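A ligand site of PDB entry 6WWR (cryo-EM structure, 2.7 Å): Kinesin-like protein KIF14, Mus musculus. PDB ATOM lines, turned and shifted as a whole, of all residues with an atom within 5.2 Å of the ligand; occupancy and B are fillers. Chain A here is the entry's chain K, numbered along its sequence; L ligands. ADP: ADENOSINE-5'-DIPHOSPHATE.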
ATOM      1  N   ARG A  14     -31.747 -27.047 -12.504  1.00  0.00           N
ATOM      2  CA  ARG A  14     -31.418 -26.256 -13.689  1.00  0.00           C
ATOM      3  C   ARG A  14     -29.967 -26.535 -14.054  1.00  0.00           C
ATOM      4  O   ARG A  14     -29.053 -26.234 -13.290  1.00  0.00           O
ATOM      5  CB  ARG A  14     -31.653 -24.784 -13.445  1.00  0.00           C
ATOM      6  CG  ARG A  14     -31.884 -24.001 -14.707  1.00  0.00           C
ATOM      7  CD  ARG A  14     -31.895 -22.526 -14.447  1.00  0.00           C
ATOM      8  NE  ARG A  14     -32.341 -21.776 -15.616  1.00  0.00           N
ATOM      9  CZ  ARG A  14     -32.350 -20.451 -15.719  1.00  0.00           C
ATOM     10  NH1 ARG A  14     -31.913 -19.694 -14.723  1.00  0.00           N
ATOM     11  NH2 ARG A  14     -32.779 -19.888 -16.829  1.00  0.00           N
ATOM     12  N   ARG A  16     -26.884 -25.502 -16.153  1.00  0.00           N
ATOM     13  CA  ARG A  16     -26.402 -24.337 -16.874  1.00  0.00           C
ATOM     14  C   ARG A  16     -25.757 -24.778 -18.190  1.00  0.00           C
ATOM     15  O   ARG A  16     -25.255 -25.892 -18.299  1.00  0.00           O
ATOM     16  CB  ARG A  16     -25.425 -23.543 -16.023  1.00  0.00           C
ATOM     17  CG  ARG A  16     -24.047 -24.125 -15.734  1.00  0.00           C
ATOM     18  CD  ARG A  16     -23.075 -22.994 -15.472  1.00  0.00           C
ATOM     19  NE  ARG A  16     -21.776 -23.424 -14.965  1.00  0.00           N
ATOM     20  CZ  ARG A  16     -20.846 -24.041 -15.689  1.00  0.00           C
ATOM     21  NH1 ARG A  16     -21.047 -24.333 -16.965  1.00  0.00           N
ATOM     22  NH2 ARG A  16     -19.700 -24.370 -15.122  1.00  0.00           N
ATOM     23  N   PRO A  17     -25.755 -23.923 -19.206  1.00  0.00           N
ATOM     24  CA  PRO A  17     -25.064 -24.260 -20.447  1.00  0.00           C
ATOM     25  C   PRO A  17     -23.568 -24.090 -20.265  1.00  0.00           C
ATOM     26  O   PRO A  17     -23.095 -23.479 -19.311  1.00  0.00           O
ATOM     27  CB  PRO A  17     -25.642 -23.240 -21.421  1.00  0.00           C
ATOM     28  CG  PRO A  17     -25.809 -22.057 -20.588  1.00  0.00           C
ATOM     29  CD  PRO A  17     -26.349 -22.573 -19.296  1.00  0.00           C
ATOM     30  N   SER A  59     -31.541 -26.008 -19.605  1.00  0.00           N
ATOM     31  CA  SER A  59     -31.022 -24.776 -20.179  1.00  0.00           C
ATOM     32  C   SER A  59     -29.653 -25.014 -20.818  1.00  0.00           C
ATOM     33  O   SER A  59     -28.745 -24.194 -20.715  1.00  0.00           O
ATOM     34  CB  SER A  59     -30.935 -23.678 -19.127  1.00  0.00           C
ATOM     35  OG  SER A  59     -29.977 -23.994 -18.128  1.00  0.00           O
ATOM     36  N   TYR A  67     -36.571 -26.401 -23.833  1.00  0.00           N
ATOM     37  CA  TYR A  67     -35.610 -25.439 -23.323  1.00  0.00           C
ATOM     38  C   TYR A  67     -36.221 -24.696 -22.147  1.00  0.00           C
ATOM     39  O   TYR A  67     -37.419 -24.383 -22.149  1.00  0.00           O
ATOM     40  CB  TYR A  67     -35.209 -24.461 -24.414  1.00  0.00           C
ATOM     41  CG  TYR A  67     -34.152 -23.476 -23.980  1.00  0.00           C
ATOM     42  CD1 TYR A  67     -32.880 -23.902 -23.630  1.00  0.00           C
ATOM     43  CD2 TYR A  67     -34.413 -22.118 -23.923  1.00  0.00           C
ATOM     44  CE1 TYR A  67     -31.911 -23.015 -23.244  1.00  0.00           C
ATOM     45  CE2 TYR A  67     -33.448 -21.224 -23.530  1.00  0.00           C
ATOM     46  CZ  TYR A  67     -32.200 -21.670 -23.195  1.00  0.00           C
ATOM     47  OH  TYR A  67     -31.231 -20.782 -22.809  1.00  0.00           O
ATOM     48  N   GLN A  98     -23.738 -24.596  -5.912  1.00  0.00           N
ATOM     49  CA  GLN A  98     -22.317 -24.346  -5.686  1.00  0.00           C
ATOM     50  C   GLN A  98     -21.829 -23.255  -6.624  1.00  0.00           C
ATOM     51  O   GLN A  98     -22.528 -22.833  -7.554  1.00  0.00           O
ATOM     52  CB  GLN A  98     -21.507 -25.615  -5.897  1.00  0.00           C
ATOM     53  CG  GLN A  98     -21.925 -26.782  -5.024  1.00  0.00           C
ATOM     54  CD  GLN A  98     -21.679 -26.549  -3.559  1.00  0.00           C
ATOM     55  OE1 GLN A  98     -22.610 -26.472  -2.762  1.00  0.00           O
ATOM     56  NE2 GLN A  98     -20.414 -26.408  -3.193  1.00  0.00           N
ATOM     57  N   THR A  99     -20.618 -22.780  -6.366  1.00  0.00           N
ATOM     58  CA  THR A  99     -20.063 -21.678  -7.131  1.00  0.00           C
ATOM     59  C   THR A  99     -19.828 -22.077  -8.571  1.00  0.00           C
ATOM     60  O   THR A  99     -19.264 -23.139  -8.864  1.00  0.00           O
ATOM     61  CB  THR A  99     -18.754 -21.217  -6.494  1.00  0.00           C
ATOM     62  OG1 THR A  99     -18.935 -21.020  -5.093  1.00  0.00           O
ATOM     63  CG2 THR A  99     -18.281 -19.926  -7.122  1.00  0.00           C
ATOM     64  N   GLY A 100     -20.263 -21.228  -9.489  1.00  0.00           N
ATOM     65  CA  GLY A 100     -20.128 -21.496 -10.903  1.00  0.00           C
ATOM     66  C   GLY A 100     -21.176 -22.428 -11.439  1.00  0.00           C
ATOM     67  O   GLY A 100     -20.850 -23.343 -12.221  1.00  0.00           O
ATOM     68  N   SER A 101     -22.440 -22.244 -11.041  1.00  0.00           N
ATOM     69  CA  SER A 101     -23.532 -23.120 -11.432  1.00  0.00           C
ATOM     70  C   SER A 101     -24.788 -22.385 -11.880  1.00  0.00           C
ATOM     71  O   SER A 101     -25.671 -23.023 -12.444  1.00  0.00           O
ATOM     72  CB  SER A 101     -23.887 -24.058 -10.284  1.00  0.00           C
ATOM     73  OG  SER A 101     -24.235 -23.329  -9.125  1.00  0.00           O
ATOM     74  N   GLY A 102     -24.890 -21.087 -11.630  1.00  0.00           N
ATOM     75  CA  GLY A 102     -26.021 -20.302 -12.097  1.00  0.00           C
ATOM     76  C   GLY A 102     -27.070 -20.056 -11.035  1.00  0.00           C
ATOM     77  O   GLY A 102     -28.275 -20.144 -11.317  1.00  0.00           O
ATOM     78  N   LYS A 103     -26.631 -19.728  -9.822  1.00  0.00           N
ATOM     79  CA  LYS A 103     -27.570 -19.363  -8.775  1.00  0.00           C
ATOM     80  C   LYS A 103     -28.083 -17.939  -8.950  1.00  0.00           C
ATOM     81  O   LYS A 103     -29.293 -17.709  -8.857  1.00  0.00           O
ATOM     82  CB  LYS A 103     -26.905 -19.512  -7.405  1.00  0.00           C
ATOM     83  CG  LYS A 103     -27.881 -19.740  -6.277  1.00  0.00           C
ATOM     84  CD  LYS A 103     -27.282 -19.440  -4.929  1.00  0.00           C
ATOM     85  CE  LYS A 103     -26.416 -20.571  -4.443  1.00  0.00           C
ATOM     86  NZ  LYS A 103     -25.339 -20.089  -3.546  1.00  0.00           N
ATOM     87  N   SER A 104     -27.191 -16.997  -9.207  1.00  0.00           N
ATOM     88  CA  SER A 104     -27.557 -15.600  -9.333  1.00  0.00           C
ATOM     89  C   SER A 104     -28.090 -15.245 -10.722  1.00  0.00           C
ATOM     90  O   SER A 104     -28.542 -14.114 -10.909  1.00  0.00           O
ATOM     91  CB  SER A 104     -26.370 -14.718  -9.002  1.00  0.00           C
ATOM     92  OG  SER A 104     -26.038 -14.827  -7.625  1.00  0.00           O
ATOM     93  N   TYR A 105     -28.044 -16.172 -11.670  1.00  0.00           N
ATOM     94  CA  TYR A 105     -28.725 -16.003 -12.950  1.00  0.00           C
ATOM     95  C   TYR A 105     -30.187 -16.431 -12.879  1.00  0.00           C
ATOM     96  O   TYR A 105     -31.019 -15.854 -13.587  1.00  0.00           O
ATOM     97  CB  TYR A 105     -27.993 -16.788 -14.035  1.00  0.00           C
ATOM     98  CG  TYR A 105     -28.608 -16.754 -15.419  1.00  0.00           C
ATOM     99  CD1 TYR A 105     -29.598 -17.648 -15.784  1.00  0.00           C
ATOM    100  CD2 TYR A 105     -28.169 -15.844 -16.364  1.00  0.00           C
ATOM    101  CE1 TYR A 105     -30.151 -17.612 -17.053  1.00  0.00           C
ATOM    102  CE2 TYR A 105     -28.715 -15.802 -17.619  1.00  0.00           C
ATOM    103  CZ  TYR A 105     -29.706 -16.694 -17.956  1.00  0.00           C
ATOM    104  OH  TYR A 105     -30.255 -16.663 -19.217  1.00  0.00           O
ATOM    105  N   LEU A 110     -29.181 -10.901 -14.824  1.00  0.00           N
ATOM    106  CA  LEU A 110     -28.347  -9.835 -15.351  1.00  0.00           C
ATOM    107  C   LEU A 110     -29.212  -8.608 -15.608  1.00  0.00           C
ATOM    108  O   LEU A 110     -30.375  -8.557 -15.172  1.00  0.00           O
ATOM    109  CB  LEU A 110     -27.620 -10.334 -16.605  1.00  0.00           C
ATOM    110  CG  LEU A 110     -26.688 -11.532 -16.403  1.00  0.00           C
ATOM    111  CD1 LEU A 110     -26.390 -12.178 -17.730  1.00  0.00           C
ATOM    112  CD2 LEU A 110     -25.413 -11.110 -15.709  1.00  0.00           C
ATOM    113  N   ASN A 214     -13.153 -20.060  -5.622  1.00  0.00           N
ATOM    114  CA  ASN A 214     -13.519 -18.858  -6.341  1.00  0.00           C
ATOM    115  C   ASN A 214     -13.031 -17.640  -5.556  1.00  0.00           C
ATOM    116  O   ASN A 214     -12.834 -17.704  -4.341  1.00  0.00           O
ATOM    117  CB  ASN A 214     -15.034 -18.787  -6.571  1.00  0.00           C
ATOM    118  CG  ASN A 214     -15.444 -17.642  -7.480  1.00  0.00           C
ATOM    119  OD1 ASN A 214     -16.233 -16.781  -7.088  1.00  0.00           O
ATOM    120  ND2 ASN A 214     -14.923 -17.626  -8.701  1.00  0.00           N
HETATM  121  PB  ADP L   1     -22.396 -17.992  -8.538  1.00  0.00           P
HETATM  122  O1B ADP L   1     -23.166 -19.254  -8.800  1.00  0.00           O
HETATM  123  O2B ADP L   1     -23.233 -16.870  -7.975  1.00  0.00           O
HETATM  124  O3B ADP L   1     -21.072 -18.192  -7.842  1.00  0.00           O
HETATM  125  PA  ADP L   1     -23.149 -17.001 -11.004  1.00  0.00           P
HETATM  126  O1A ADP L   1     -24.244 -18.023 -10.936  1.00  0.00           O
HETATM  127  O2A ADP L   1     -23.471 -15.549 -10.727  1.00  0.00           O
HETATM  128  O3A ADP L   1     -21.988 -17.483 -10.005  1.00  0.00           O
HETATM  129  O5' ADP L   1     -22.485 -17.106 -12.455  1.00  0.00           O
HETATM  130  C5' ADP L   1     -23.270 -17.738 -13.469  1.00  0.00           C
HETATM  131  C4' ADP L   1     -22.716 -17.469 -14.863  1.00  0.00           C
HETATM  132  O4' ADP L   1     -23.171 -18.515 -15.718  1.00  0.00           O
HETATM  133  C3' ADP L   1     -23.177 -16.143 -15.457  1.00  0.00           C
HETATM  134  O3' ADP L   1     -22.045 -15.366 -15.853  1.00  0.00           O
HETATM  135  C2' ADP L   1     -24.032 -16.503 -16.655  1.00  0.00           C
HETATM  136  O2' ADP L   1     -23.593 -15.806 -17.832  1.00  0.00           O
HETATM  137  C1' ADP L   1     -23.867 -17.998 -16.851  1.00  0.00           C
HETATM  138  N9  ADP L   1     -25.178 -18.672 -16.955  1.00  0.00           N
HETATM  139  C8  ADP L   1     -25.793 -19.320 -15.943  1.00  0.00           C
HETATM  140  N7  ADP L   1     -26.975 -19.847 -16.360  1.00  0.00           N
HETATM  141  C5  ADP L   1     -27.118 -19.524 -17.648  1.00  0.00           C
HETATM  142  C6  ADP L   1     -28.134 -19.774 -18.694  1.00  0.00           C
HETATM  143  N6  ADP L   1     -29.249 -20.474 -18.400  1.00  0.00           N
HETATM  144  N1  ADP L   1     -27.910 -19.272 -19.920  1.00  0.00           N
HETATM  145  C2  ADP L   1     -26.795 -18.572 -20.214  1.00  0.00           C
HETATM  146  N3  ADP L   1     -25.832 -18.320 -19.311  1.00  0.00           N
HETATM  147  C4  ADP L   1     -25.937 -18.763 -18.042  1.00  0.00           C
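O1A of the ligand lies within hydrogen-bond range of N of Lys 103.
An oxygen (O1A) of the ligand sits close to the backbone NH (N) of Gly 102 (3.2 Å).
The side-chain hydroxyl (OG) of Ser 104 lies within hydrogen-bond range of an oxygen (O2B) of the ligand, 3.5 Å away.
N of Gln 98 lies close to OG of Ser 101 (3.5 Å).
NE of Arg 16 sits at hydrogen-bond distance from O of Gly 100 (2.9 Å).
NH2 of Arg 14 touches N6 of the ligand, at 3.9 Å.
Pro 17 touches the ligand.
OG of Ser 59 touches N6 of the ligand, 3.6 Å away.
O of Gln 98 touches O1B of the ligand (3.8 Å).
Thr 99 touches the ligand (CG2 to O3B, 3.4 Å).
Gly 100 touches the ligand (N to O3B, 3.5 Å).
Ser 101 touches the ligand.
Tyr 105 touches the ligand.
Hydrophobic or aromatic side chains within 4 Å of the ligand: Pro 17 and Tyr 105.
Within 4 Å of the ligand: Arg 14, Pro 17, Ser 59, Gln 98, Thr 99, Gly 100, Ser 101, Gly 102, Lys 103, Ser 104 and Tyr 105.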
